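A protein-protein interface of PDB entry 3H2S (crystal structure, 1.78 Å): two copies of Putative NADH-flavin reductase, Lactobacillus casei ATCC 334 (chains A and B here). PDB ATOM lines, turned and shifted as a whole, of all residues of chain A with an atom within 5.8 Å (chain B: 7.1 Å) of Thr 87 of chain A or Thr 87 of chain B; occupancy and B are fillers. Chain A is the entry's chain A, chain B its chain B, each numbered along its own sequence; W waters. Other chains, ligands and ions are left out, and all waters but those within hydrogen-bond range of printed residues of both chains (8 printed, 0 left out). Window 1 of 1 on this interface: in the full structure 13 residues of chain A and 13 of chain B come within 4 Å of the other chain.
The backbone carbonyl oxygen (O) of Leu 145 of chain B lies close to the side-chain amide oxygen (OD1) of Asn 148 of chain B (3.5 Å).
The side-chain amide oxygen (OD1) of Asn 148 of chain B sits close to the backbone carbonyl oxygen (O) of Phe 144 of chain B (2.8 Å).
The backbone carbonyl oxygen of His 88 of chain A sits at hydrogen-bond distance from the side-chain hydroxyl of Ser 91 of chain A, 2.6 Å away.
The side-chain hydroxyl (OG) of Ser 91 of chain B is in hydrogen-bond range of the backbone carbonyl oxygen (O) of His 88 of chain B (2.6 Å).
OG1 of Thr 87 of chain B lies close to O of Leu 83 of chain B, 3.4 Å away.
O of Asp 84 of chain B is in hydrogen-bond range of OG1 of Thr 87 of chain B (3.1 Å).
NH2 of Arg 94 of chain B lies within salt-bridge range of OD1 of Asp 84 of chain A.
Water W5 lies within hydrogen-bond range of the side-chain carboxylate (OD1) of Asp 84 of chain A (2.7 Å), the backbone carbonyl oxygen (O) of Thr 87 of chain B (2.8 Å) and the side-chain hydroxyl (OG1) of Thr 87 of chain A (2.8 Å).
Water W6 lies within hydrogen-bond range of OG1 of Thr 87 of chain B (2.7 Å), OD1 of Asp 84 of chain B (2.7 Å) and O of Thr 87 of chain A (2.9 Å).
Water W7 bridges the side-chain carboxylate (OD2) of Asp 84 of chain A (2.7 Å) and the backbone carbonyl oxygen (O) of Ser 91 of chain B (2.8 Å).
Water W1 lies within hydrogen-bond range of OG1 of Thr 87 of chain A (2.9 Å), OG1 of Thr 87 of chain B (3.1 Å), N of His 88 of chain A (3.3 Å) and N of His 88 of chain B (3.4 Å).
Water W3 lies within hydrogen-bond range of ND1 of His 88 of chain B (2.9 Å), OG of Ser 91 of chain B (3.1 Å) and ND1 of His 88 of chain A (3.2 Å).
Water W2 lies within hydrogen-bond range of O of Asp 84 of chain B (2.9 Å), OG1 of Thr 87 of chain B (3.1 Å) and OG of Ser 91 of chain A (3.3 Å).
CD2 of Leu 83 of chain A touches CE1 of Phe 144 of chain B, at 3.8 Å.
Asn 148 of chain B touches Leu 83 of chain A (ND2 to CD2, 3.9 Å).
Ser 91 of chain B touches Asp 84 of chain A (CA to OD2, 3.7 Å).
Thr 87 of chain A touches Thr 87 of chain B (CB to CB, 3.5 Å).
Asp 84 of chain B touches Ser 91 of chain A.
CD2 of Leu 83 of chain B touches CE1 of Phe 144 of chain A, 3.7 Å away.
Printed residues of chain B within 4 Å of Thr 87 of chain A: Thr 87.
Printed residues of chain B within 4 Å of Ser 91 of chain A: Asp 84.
Printed residues of chain B within 4 Å of Asp 84 of chain A: Ser 91 and Arg 94.
Of the printed residues of chain B, Leu 83 of chain A touches Phe 144 and Asn 148.
Leu 92 of chain A touches none of the printed residues of chain B.
The nearest residue of chain A that does not touch Thr 87 of chain B is Phe 144 of chain A (4.1 Å).
The nearest printed residue of chain A that does not touch Asn 148 of chain B is Asp 84 of chain A (5.4 Å).
Leu 83 of chain A touches Phe 144 of chain B, and with the chains exchanged Phe 144 of chain A touches Leu 83 of chain B.
Asp 84 of chain A touches Ser 91 of chain B, and with the chains exchanged Ser 91 of chain A touches Asp 84 of chain B.
Thr 87 of chain B touches its own counterpart, Thr 87 of chain A.
Positions printed for both chains: 82, 83, 84, 85, 86, 87, 88, 89, 90, 91, 92 and 144.
Of the 7 pairs that touch across the chains among the printed residues, 5 have their exchanged pair printed and touching as well.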
ATOM      1  N   HIS A  82      -4.658  -7.238  24.554  1.00  0.00           N
ATOM      2  CA  HIS A  82      -3.772  -8.145  23.838  1.00  0.00           C
ATOM      3  C   HIS A  82      -4.366  -8.502  22.480  1.00  0.00           C
ATOM      4  O   HIS A  82      -3.668  -8.515  21.456  1.00  0.00           O
ATOM      5  CB  HIS A  82      -3.541  -9.419  24.643  1.00  0.00           C
ATOM      6  CG  HIS A  82      -2.516  -9.268  25.723  1.00  0.00           C
ATOM      7  ND1 HIS A  82      -2.827  -9.355  27.062  1.00  0.00           N
ATOM      8  CD2 HIS A  82      -1.184  -9.036  25.657  1.00  0.00           C
ATOM      9  CE1 HIS A  82      -1.710  -9.289  27.770  1.00  0.00           C
ATOM     10  NE2 HIS A  82      -0.704  -9.071  26.942  1.00  0.00           N
ATOM     11  N   LEU A  83      -5.646  -8.850  22.494  1.00  0.00           N
ATOM     12  CA  LEU A  83      -6.369  -9.162  21.275  1.00  0.00           C
ATOM     13  C   LEU A  83      -6.605  -7.939  20.372  1.00  0.00           C
ATOM     14  O   LEU A  83      -6.265  -7.964  19.184  1.00  0.00           O
ATOM     15  CB  LEU A  83      -7.687  -9.854  21.609  1.00  0.00           C
ATOM     16  CG  LEU A  83      -8.572 -10.324  20.448  1.00  0.00           C
ATOM     17  CD1 LEU A  83      -7.807 -11.278  19.496  1.00  0.00           C
ATOM     18  CD2 LEU A  83      -9.820 -10.991  21.001  1.00  0.00           C
ATOM     19  N   ASP A  84      -7.157  -6.869  20.941  1.00  0.00           N
ATOM     20  CA  ASP A  84      -7.497  -5.666  20.174  1.00  0.00           C
ATOM     21  C   ASP A  84      -6.287  -5.032  19.484  1.00  0.00           C
ATOM     22  O   ASP A  84      -6.388  -4.589  18.343  1.00  0.00           O
ATOM     23  CB  ASP A  84      -8.199  -4.631  21.071  1.00  0.00           C
ATOM     24  CG  ASP A  84      -9.633  -5.028  21.420  1.00  0.00           C
ATOM     25  OD1 ASP A  84     -10.205  -5.950  20.783  1.00  0.00           O
ATOM     26  OD2 ASP A  84     -10.184  -4.430  22.367  1.00  0.00           O
ATOM     27  N   PHE A  85      -5.155  -4.931  20.175  1.00  0.00           N
ATOM     28  CA  PHE A  85      -3.966  -4.362  19.520  1.00  0.00           C
ATOM     29  C   PHE A  85      -3.611  -5.207  18.282  1.00  0.00           C
ATOM     30  O   PHE A  85      -3.186  -4.671  17.259  1.00  0.00           O
ATOM     31  CB  PHE A  85      -2.769  -4.362  20.465  1.00  0.00           C
ATOM     32  CG  PHE A  85      -2.939  -3.494  21.691  1.00  0.00           C
ATOM     33  CD1 PHE A  85      -3.413  -2.191  21.582  1.00  0.00           C
ATOM     34  CD2 PHE A  85      -2.395  -3.898  22.900  1.00  0.00           C
ATOM     35  CE1 PHE A  85      -3.387  -1.328  22.662  1.00  0.00           C
ATOM     36  CE2 PHE A  85      -2.381  -3.025  23.998  1.00  0.00           C
ATOM     37  CZ  PHE A  85      -2.920  -1.761  23.877  1.00  0.00           C
ATOM     38  N   ALA A  86      -3.636  -6.537  18.431  1.00  0.00           N
ATOM     39  CA  ALA A  86      -3.250  -7.418  17.337  1.00  0.00           C
ATOM     40  C   ALA A  86      -4.216  -7.343  16.157  1.00  0.00           C
ATOM     41  O   ALA A  86      -3.778  -7.333  14.998  1.00  0.00           O
ATOM     42  CB  ALA A  86      -3.105  -8.867  17.834  1.00  0.00           C
ATOM     43  N   THR A  87      -5.520  -7.403  16.435  1.00  0.00           N
ATOM     44  CA  THR A  87      -6.508  -7.336  15.354  1.00  0.00           C
ATOM     45  C   THR A  87      -6.360  -6.010  14.620  1.00  0.00           C
ATOM     46  O   THR A  87      -6.528  -5.947  13.404  1.00  0.00           O
ATOM     47  CB  THR A  87      -7.964  -7.481  15.864  1.00  0.00           C
ATOM     48  OG1 THR A  87      -8.295  -6.370  16.716  1.00  0.00           O
ATOM     49  CG2 THR A  87      -8.168  -8.817  16.640  1.00  0.00           C
ATOM     50  N   HIS A  88      -6.092  -4.936  15.364  1.00  0.00           N
ATOM     51  CA  HIS A  88      -5.938  -3.632  14.729  1.00  0.00           C
ATOM     52  C   HIS A  88      -4.706  -3.628  13.829  1.00  0.00           C
ATOM     53  O   HIS A  88      -4.751  -3.137  12.692  1.00  0.00           O
ATOM     54  CB  HIS A  88      -5.829  -2.509  15.773  1.00  0.00           C
ATOM     55  CG  HIS A  88      -5.797  -1.140  15.166  1.00  0.00           C
ATOM     56  ND1 HIS A  88      -6.808  -0.677  14.352  1.00  0.00           N
ATOM     57  CD2 HIS A  88      -4.799  -0.225  15.084  1.00  0.00           C
ATOM     58  CE1 HIS A  88      -6.479   0.516  13.882  1.00  0.00           C
ATOM     59  NE2 HIS A  88      -5.252   0.796  14.282  1.00  0.00           N
ATOM     60  N   LEU A  89      -3.584  -4.103  14.363  1.00  0.00           N
ATOM     61  CA  LEU A  89      -2.347  -4.169  13.563  1.00  0.00           C
ATOM     62  C   LEU A  89      -2.516  -4.978  12.272  1.00  0.00           C
ATOM     63  O   LEU A  89      -2.103  -4.546  11.190  1.00  0.00           O
ATOM     64  CB  LEU A  89      -1.187  -4.738  14.393  1.00  0.00           C
ATOM     65  CG  LEU A  89       0.165  -4.762  13.661  1.00  0.00           C
ATOM     66  CD1 LEU A  89       0.489  -3.422  12.976  1.00  0.00           C
ATOM     67  CD2 LEU A  89       1.303  -5.185  14.592  1.00  0.00           C
ATOM     68  N   VAL A  90      -3.068  -6.182  12.398  1.00  0.00           N
ATOM     69  CA  VAL A  90      -3.372  -7.007  11.228  1.00  0.00           C
ATOM     70  C   VAL A  90      -4.217  -6.258  10.191  1.00  0.00           C
ATOM     71  O   VAL A  90      -3.951  -6.328   8.984  1.00  0.00           O
ATOM     72  CB  VAL A  90      -4.037  -8.355  11.626  1.00  0.00           C
ATOM     73  CG1 VAL A  90      -4.605  -9.073  10.385  1.00  0.00           C
ATOM     74  CG2 VAL A  90      -3.006  -9.259  12.329  1.00  0.00           C
ATOM     75  N   SER A  91      -5.171  -5.462  10.654  1.00  0.00           N
ATOM     76  CA  SER A  91      -6.054  -4.760   9.732  1.00  0.00           C
ATOM     77  C   SER A  91      -5.305  -3.726   8.901  1.00  0.00           C
ATOM     78  O   SER A  91      -5.751  -3.359   7.813  1.00  0.00           O
ATOM     79  CB  SER A  91      -7.211  -4.103  10.484  1.00  0.00           C
ATOM     80  OG  SER A  91      -6.814  -2.871  11.072  1.00  0.00           O
ATOM     81  N   LEU A  92      -4.139  -3.297   9.389  1.00  0.00           N
ATOM     82  CA  LEU A  92      -3.330  -2.294   8.684  1.00  0.00           C
ATOM     83  C   LEU A  92      -2.353  -2.961   7.723  1.00  0.00           C
ATOM     84  O   LEU A  92      -1.642  -2.282   6.989  1.00  0.00           O
ATOM     85  CB  LEU A  92      -2.536  -1.442   9.684  1.00  0.00           C
ATOM     86  CG  LEU A  92      -3.321  -0.773  10.811  1.00  0.00           C
ATOM     87  CD1 LEU A  92      -2.375  -0.034  11.754  1.00  0.00           C
ATOM     88  CD2 LEU A  92      -4.346   0.195  10.204  1.00  0.00           C
ATOM     89  N   PHE A 144      -6.342 -15.952  16.709  1.00  0.00           N
ATOM     90  CA  PHE A 144      -6.726 -14.935  15.722  1.00  0.00           C
ATOM     91  C   PHE A 144      -5.693 -14.827  14.603  1.00  0.00           C
ATOM     92  O   PHE A 144      -6.039 -14.715  13.431  1.00  0.00           O
ATOM     93  CB  PHE A 144      -6.889 -13.565  16.375  1.00  0.00           C
ATOM     94  CG  PHE A 144      -6.915 -12.439  15.387  1.00  0.00           C
ATOM     95  CD1 PHE A 144      -8.056 -12.176  14.653  1.00  0.00           C
ATOM     96  CD2 PHE A 144      -5.782 -11.653  15.169  1.00  0.00           C
ATOM     97  CE1 PHE A 144      -8.071 -11.177  13.678  1.00  0.00           C
ATOM     98  CE2 PHE A 144      -5.807 -10.609  14.254  1.00  0.00           C
ATOM     99  CZ  PHE A 144      -6.940 -10.390  13.485  1.00  0.00           C
ATOM    100  N   LEU B  53     -13.468   1.336   9.340  1.00  0.00           N
ATOM    101  CA  LEU B  53     -12.258   0.981  10.063  1.00  0.00           C
ATOM    102  C   LEU B  53     -11.630   2.175  10.783  1.00  0.00           C
ATOM    103  O   LEU B  53     -10.725   1.998  11.583  1.00  0.00           O
ATOM    104  CB  LEU B  53     -11.228   0.330   9.136  1.00  0.00           C
ATOM    105  CG  LEU B  53     -11.199  -1.199   9.066  1.00  0.00           C
ATOM    106  CD1 LEU B  53     -12.291  -1.905   9.843  1.00  0.00           C
ATOM    107  CD2 LEU B  53     -11.073  -1.738   7.657  1.00  0.00           C
ATOM    108  N   ASP B  68     -23.934  -4.432  12.353  1.00  0.00           N
ATOM    109  CA  ASP B  68     -22.949  -4.634  11.285  1.00  0.00           C
ATOM    110  C   ASP B  68     -23.627  -5.306  10.093  1.00  0.00           C
ATOM    111  O   ASP B  68     -23.818  -6.526  10.078  1.00  0.00           O
ATOM    112  CB  ASP B  68     -21.770  -5.486  11.792  1.00  0.00           C
ATOM    113  CG  ASP B  68     -20.721  -5.746  10.719  1.00  0.00           C
ATOM    114  OD1 ASP B  68     -20.918  -5.332   9.548  1.00  0.00           O
ATOM    115  OD2 ASP B  68     -19.658  -6.309  11.072  1.00  0.00           O
ATOM    116  N   TYR B  80     -11.363 -10.572   3.797  1.00  0.00           N
ATOM    117  CA  TYR B  80     -10.819 -10.264   5.136  1.00  0.00           C
ATOM    118  C   TYR B  80     -11.566  -9.126   5.844  1.00  0.00           C
ATOM    119  O   TYR B  80     -11.503  -9.000   7.071  1.00  0.00           O
ATOM    120  CB  TYR B  80      -9.316  -9.960   5.090  1.00  0.00           C
ATOM    121  CG  TYR B  80      -8.951  -8.825   4.161  1.00  0.00           C
ATOM    122  CD1 TYR B  80      -9.175  -7.501   4.527  1.00  0.00           C
ATOM    123  CD2 TYR B  80      -8.330  -9.076   2.936  1.00  0.00           C
ATOM    124  CE1 TYR B  80      -8.811  -6.460   3.688  1.00  0.00           C
ATOM    125  CE2 TYR B  80      -7.982  -8.036   2.083  1.00  0.00           C
ATOM    126  CZ  TYR B  80      -8.238  -6.733   2.462  1.00  0.00           C
ATOM    127  OH  TYR B  80      -7.894  -5.692   1.617  1.00  0.00           O
ATOM    128  N   LEU B  81     -12.230  -8.274   5.068  1.00  0.00           N
ATOM    129  CA  LEU B  81     -12.960  -7.139   5.648  1.00  0.00           C
ATOM    130  C   LEU B  81     -14.110  -7.579   6.549  1.00  0.00           C
ATOM    131  O   LEU B  81     -14.359  -6.947   7.580  1.00  0.00           O
ATOM    132  CB  LEU B  81     -13.484  -6.196   4.559  1.00  0.00           C
ATOM    133  CG  LEU B  81     -12.442  -5.310   3.862  1.00  0.00           C
ATOM    134  CD1 LEU B  81     -13.146  -4.408   2.827  1.00  0.00           C
ATOM    135  CD2 LEU B  81     -11.606  -4.451   4.862  1.00  0.00           C
ATOM    136  N   HIS B  82     -14.730  -8.720   6.252  1.00  0.00           N
ATOM    137  CA  HIS B  82     -15.735  -9.273   7.171  1.00  0.00           C
ATOM    138  C   HIS B  82     -15.178  -9.375   8.593  1.00  0.00           C
ATOM    139  O   HIS B  82     -15.827  -8.985   9.572  1.00  0.00           O
ATOM    140  CB  HIS B  82     -16.202 -10.645   6.707  1.00  0.00           C
ATOM    141  CG  HIS B  82     -17.234 -10.592   5.628  1.00  0.00           C
ATOM    142  ND1 HIS B  82     -17.006 -11.068   4.353  1.00  0.00           N
ATOM    143  CD2 HIS B  82     -18.498 -10.106   5.631  1.00  0.00           C
ATOM    144  CE1 HIS B  82     -18.116 -10.949   3.642  1.00  0.00           C
ATOM    145  NE2 HIS B  82     -19.018 -10.323   4.379  1.00  0.00           N
ATOM    146  N   LEU B  83     -13.943  -9.847   8.690  1.00  0.00           N
ATOM    147  CA  LEU B  83     -13.269  -9.975   9.974  1.00  0.00           C
ATOM    148  C   LEU B  83     -12.808  -8.621  10.511  1.00  0.00           C
ATOM    149  O   LEU B  83     -13.083  -8.278  11.671  1.00  0.00           O
ATOM    150  CB  LEU B  83     -12.091 -10.939   9.848  1.00  0.00           C
ATOM    151  CG  LEU B  83     -11.314 -11.288  11.128  1.00  0.00           C
ATOM    152  CD1 LEU B  83     -12.239 -11.940  12.177  1.00  0.00           C
ATOM    153  CD2 LEU B  83     -10.172 -12.235  10.763  1.00  0.00           C
ATOM    154  N   ASP B  84     -12.122  -7.849   9.671  1.00  0.00           N
ATOM    155  CA  ASP B  84     -11.583  -6.558  10.099  1.00  0.00           C
ATOM    156  C   ASP B  84     -12.641  -5.591  10.607  1.00  0.00           C
ATOM    157  O   ASP B  84     -12.403  -4.877  11.586  1.00  0.00           O
ATOM    158  CB  ASP B  84     -10.739  -5.902   9.000  1.00  0.00           C
ATOM    159  CG  ASP B  84      -9.387  -6.587   8.807  1.00  0.00           C
ATOM    160  OD1 ASP B  84      -8.963  -7.380   9.682  1.00  0.00           O
ATOM    161  OD2 ASP B  84      -8.786  -6.393   7.740  1.00  0.00           O
ATOM    162  N   PHE B  85     -13.801  -5.543   9.948  1.00  0.00           N
ATOM    163  CA  PHE B  85     -14.850  -4.618  10.395  1.00  0.00           C
ATOM    164  C   PHE B  85     -15.359  -5.039  11.777  1.00  0.00           C
ATOM    165  O   PHE B  85     -15.601  -4.201  12.638  1.00  0.00           O
ATOM    166  CB  PHE B  85     -16.036  -4.601   9.420  1.00  0.00           C
ATOM    167  CG  PHE B  85     -15.714  -4.051   8.055  1.00  0.00           C
ATOM    168  CD1 PHE B  85     -15.001  -2.870   7.912  1.00  0.00           C
ATOM    169  CD2 PHE B  85     -16.316  -4.600   6.939  1.00  0.00           C
ATOM    170  CE1 PHE B  85     -14.839  -2.278   6.659  1.00  0.00           C
ATOM    171  CE2 PHE B  85     -16.176  -4.014   5.681  1.00  0.00           C
ATOM    172  CZ  PHE B  85     -15.383  -2.879   5.535  1.00  0.00           C
ATOM    173  N   ALA B  86     -15.526  -6.348  11.978  1.00  0.00           N
ATOM    174  CA  ALA B  86     -16.012  -6.875  13.252  1.00  0.00           C
ATOM    175  C   ALA B  86     -15.007  -6.703  14.388  1.00  0.00           C
ATOM    176  O   ALA B  86     -15.386  -6.327  15.503  1.00  0.00           O
ATOM    177  CB  ALA B  86     -16.407  -8.350  13.099  1.00  0.00           C
ATOM    178  N   THR B  87     -13.725  -6.940  14.115  1.00  0.00           N
ATOM    179  CA  THR B  87     -12.721  -6.807  15.172  1.00  0.00           C
ATOM    180  C   THR B  87     -12.586  -5.337  15.573  1.00  0.00           C
ATOM    181  O   THR B  87     -12.386  -5.033  16.743  1.00  0.00           O
ATOM    182  CB  THR B  87     -11.328  -7.348  14.762  1.00  0.00           C
ATOM    183  OG1 THR B  87     -10.816  -6.598  13.642  1.00  0.00           O
ATOM    184  CG2 THR B  87     -11.406  -8.824  14.392  1.00  0.00           C
ATOM    185  N   HIS B  88     -12.659  -4.431  14.594  1.00  0.00           N
ATOM    186  CA  HIS B  88     -12.642  -3.002  14.899  1.00  0.00           C
ATOM    187  C   HIS B  88     -13.849  -2.593  15.737  1.00  0.00           C
ATOM    188  O   HIS B  88     -13.701  -1.918  16.757  1.00  0.00           O
ATOM    189  CB  HIS B  88     -12.560  -2.153  13.620  1.00  0.00           C
ATOM    190  CG  HIS B  88     -12.344  -0.690  13.886  1.00  0.00           C
ATOM    191  ND1 HIS B  88     -11.223  -0.211  14.534  1.00  0.00           N
ATOM    192  CD2 HIS B  88     -13.181   0.367  13.757  1.00  0.00           C
ATOM    193  CE1 HIS B  88     -11.360   1.088  14.749  1.00  0.00           C
ATOM    194  NE2 HIS B  88     -12.528   1.467  14.267  1.00  0.00           N
ATOM    195  N   LEU B  89     -15.043  -3.019  15.329  1.00  0.00           N
ATOM    196  CA  LEU B  89     -16.250  -2.662  16.079  1.00  0.00           C
ATOM    197  C   LEU B  89     -16.179  -3.141  17.530  1.00  0.00           C
ATOM    198  O   LEU B  89     -16.472  -2.377  18.458  1.00  0.00           O
ATOM    199  CB  LEU B  89     -17.512  -3.201  15.404  1.00  0.00           C
ATOM    200  CG  LEU B  89     -18.828  -2.953  16.159  1.00  0.00           C
ATOM    201  CD1 LEU B  89     -19.027  -1.464  16.438  1.00  0.00           C
ATOM    202  CD2 LEU B  89     -20.000  -3.504  15.343  1.00  0.00           C
ATOM    203  N   VAL B  90     -15.792  -4.405  17.720  1.00  0.00           N
ATOM    204  CA  VAL B  90     -15.671  -4.967  19.050  1.00  0.00           C
ATOM    205  C   VAL B  90     -14.716  -4.161  19.919  1.00  0.00           C
ATOM    206  O   VAL B  90     -14.983  -3.930  21.111  1.00  0.00           O
ATOM    207  CB  VAL B  90     -15.260  -6.462  19.001  1.00  0.00           C
ATOM    208  CG1 VAL B  90     -14.758  -6.926  20.365  1.00  0.00           C
ATOM    209  CG2 VAL B  90     -16.476  -7.312  18.567  1.00  0.00           C
ATOM    210  N   SER B  91     -13.599  -3.737  19.328  1.00  0.00           N
ATOM    211  CA  SER B  91     -12.612  -2.934  20.055  1.00  0.00           C
ATOM    212  C   SER B  91     -13.197  -1.638  20.618  1.00  0.00           C
ATOM    213  O   SER B  91     -12.646  -1.075  21.565  1.00  0.00           O
ATOM    214  CB  SER B  91     -11.379  -2.655  19.198  1.00  0.00           C
ATOM    215  OG  SER B  91     -11.602  -1.561  18.313  1.00  0.00           O
ATOM    216  N   LEU B  92     -14.284  -1.148  20.009  1.00  0.00           N
ATOM    217  CA  LEU B  92     -14.895   0.127  20.414  1.00  0.00           C
ATOM    218  C   LEU B  92     -15.940  -0.076  21.501  1.00  0.00           C
ATOM    219  O   LEU B  92     -16.424   0.887  22.105  1.00  0.00           O
ATOM    220  CB  LEU B  92     -15.551   0.822  19.216  1.00  0.00           C
ATOM    221  CG  LEU B  92     -14.656   1.119  18.006  1.00  0.00           C
ATOM    222  CD1 LEU B  92     -15.471   1.733  16.876  1.00  0.00           C
ATOM    223  CD2 LEU B  92     -13.503   2.042  18.414  1.00  0.00           C
ATOM    224  N   ARG B  94     -15.638  -2.110  24.271  1.00  0.00           N
ATOM    225  CA  ARG B  94     -15.097  -2.634  25.514  1.00  0.00           C
ATOM    226  C   ARG B  94     -15.588  -1.812  26.703  1.00  0.00           C
ATOM    227  O   ARG B  94     -15.703  -0.582  26.622  1.00  0.00           O
ATOM    228  CB  ARG B  94     -13.566  -2.641  25.481  1.00  0.00           C
ATOM    229  CG  ARG B  94     -12.981  -3.422  24.306  1.00  0.00           C
ATOM    230  CD  ARG B  94     -13.196  -4.914  24.487  1.00  0.00           C
ATOM    231  NE  ARG B  94     -12.423  -5.675  23.520  1.00  0.00           N
ATOM    232  CZ  ARG B  94     -12.607  -6.964  23.255  1.00  0.00           C
ATOM    233  NH1 ARG B  94     -13.513  -7.660  23.921  1.00  0.00           N
ATOM    234  NH2 ARG B  94     -11.902  -7.546  22.303  1.00  0.00           N
ATOM    235  N   PHE B 102     -24.312  -8.610  14.644  1.00  0.00           N
ATOM    236  CA  PHE B 102     -23.478  -8.912  13.476  1.00  0.00           C
ATOM    237  C   PHE B 102     -24.213  -9.887  12.568  1.00  0.00           C
ATOM    238  O   PHE B 102     -24.596 -10.971  12.996  1.00  0.00           O
ATOM    239  CB  PHE B 102     -22.149  -9.557  13.916  1.00  0.00           C
ATOM    240  CG  PHE B 102     -21.263  -8.635  14.710  1.00  0.00           C
ATOM    241  CD1 PHE B 102     -20.276  -7.896  14.082  1.00  0.00           C
ATOM    242  CD2 PHE B 102     -21.447  -8.479  16.081  1.00  0.00           C
ATOM    243  CE1 PHE B 102     -19.449  -7.036  14.816  1.00  0.00           C
ATOM    244  CE2 PHE B 102     -20.670  -7.575  16.814  1.00  0.00           C
ATOM    245  CZ  PHE B 102     -19.675  -6.852  16.177  1.00  0.00           C
ATOM    246  N   GLU B 141     -15.068 -14.615  11.522  1.00  0.00           N
ATOM    247  CA  GLU B 141     -15.768 -13.538  12.231  1.00  0.00           C
ATOM    248  C   GLU B 141     -16.632 -14.108  13.352  1.00  0.00           C
ATOM    249  O   GLU B 141     -16.521 -13.697  14.508  1.00  0.00           O
ATOM    250  CB  GLU B 141     -16.648 -12.731  11.261  1.00  0.00           C
ATOM    251  CG  GLU B 141     -17.442 -11.604  11.940  1.00  0.00           C
ATOM    252  CD  GLU B 141     -18.418 -10.901  10.993  1.00  0.00           C
ATOM    253  OE1 GLU B 141     -18.539 -11.319   9.810  1.00  0.00           O
ATOM    254  OE2 GLU B 141     -19.093  -9.946  11.451  1.00  0.00           O
ATOM    255  N   PHE B 144     -14.296 -15.396  16.051  1.00  0.00           N
ATOM    256  CA  PHE B 144     -13.770 -14.233  16.767  1.00  0.00           C
ATOM    257  C   PHE B 144     -14.763 -13.685  17.777  1.00  0.00           C
ATOM    258  O   PHE B 144     -14.379 -13.279  18.858  1.00  0.00           O
ATOM    259  CB  PHE B 144     -13.382 -13.122  15.798  1.00  0.00           C
ATOM    260  CG  PHE B 144     -13.169 -11.789  16.463  1.00  0.00           C
ATOM    261  CD1 PHE B 144     -12.023 -11.542  17.209  1.00  0.00           C
ATOM    262  CD2 PHE B 144     -14.148 -10.800  16.395  1.00  0.00           C
ATOM    263  CE1 PHE B 144     -11.851 -10.317  17.866  1.00  0.00           C
ATOM    264  CE2 PHE B 144     -13.944  -9.552  16.977  1.00  0.00           C
ATOM    265  CZ  PHE B 144     -12.822  -9.325  17.746  1.00  0.00           C
ATOM    266  N   LEU B 145     -16.025 -13.557  17.376  1.00  0.00           N
ATOM    267  CA  LEU B 145     -17.029 -13.029  18.287  1.00  0.00           C
ATOM    268  C   LEU B 145     -17.073 -13.800  19.610  1.00  0.00           C
ATOM    269  O   LEU B 145     -17.107 -13.204  20.693  1.00  0.00           O
ATOM    270  CB  LEU B 145     -18.402 -12.984  17.609  1.00  0.00           C
ATOM    271  CG  LEU B 145     -18.611 -11.920  16.522  1.00  0.00           C
ATOM    272  CD1 LEU B 145     -20.069 -11.992  16.030  1.00  0.00           C
ATOM    273  CD2 LEU B 145     -18.250 -10.473  16.985  1.00  0.00           C
ATOM    274  N   MET B 147     -14.759 -15.163  21.161  1.00  0.00           N
ATOM    275  CA  MET B 147     -13.617 -14.843  22.016  1.00  0.00           C
ATOM    276  C   MET B 147     -13.907 -13.719  22.996  1.00  0.00           C
ATOM    277  O   MET B 147     -13.016 -13.299  23.740  1.00  0.00           O
ATOM    278  CB  MET B 147     -12.424 -14.430  21.174  1.00  0.00           C
ATOM    279  CG  MET B 147     -12.002 -15.475  20.189  1.00  0.00           C
ATOM    280  SD  MET B 147     -10.547 -14.828  19.079  1.00  0.00           S
ATOM    281  CE  MET B 147     -10.153 -16.522  18.191  1.00  0.00           C
ATOM    282  N   ASN B 148     -15.096 -13.135  22.894  1.00  0.00           N
ATOM    283  CA  ASN B 148     -15.389 -11.896  23.620  1.00  0.00           C
ATOM    284  C   ASN B 148     -16.570 -12.010  24.589  1.00  0.00           C
ATOM    285  O   ASN B 148     -17.704 -11.658  24.252  1.00  0.00           O
ATOM    286  CB  ASN B 148     -15.604 -10.766  22.624  1.00  0.00           C
ATOM    287  CG  ASN B 148     -14.413 -10.580  21.711  1.00  0.00           C
ATOM    288  OD1 ASN B 148     -14.416 -11.025  20.561  1.00  0.00           O
ATOM    289  ND2 ASN B 148     -13.343 -10.028  22.260  1.00  0.00           N
HETATM  290  O   HOH W   1      -9.353  -4.263  15.114  1.00  0.00           O
HETATM  291  O   HOH W   2      -9.637  -4.138  12.275  1.00  0.00           O
HETATM  292  O   HOH W   3      -9.248  -1.444  16.267  1.00  0.00           O
HETATM  293  O   HOH W   4      -8.211  -3.918   6.794  1.00  0.00           O
HETATM  294  O   HOH W   5     -10.649  -6.625  18.237  1.00  0.00           O
HETATM  295  O   HOH W   6      -8.681  -7.572  12.353  1.00  0.00           O
HETATM  296  O   HOH W   7     -10.228  -1.774  22.824  1.00  0.00           O
HETATM  297  O   HOH W   8      -8.856  -1.751  12.828  1.00  0.00           O
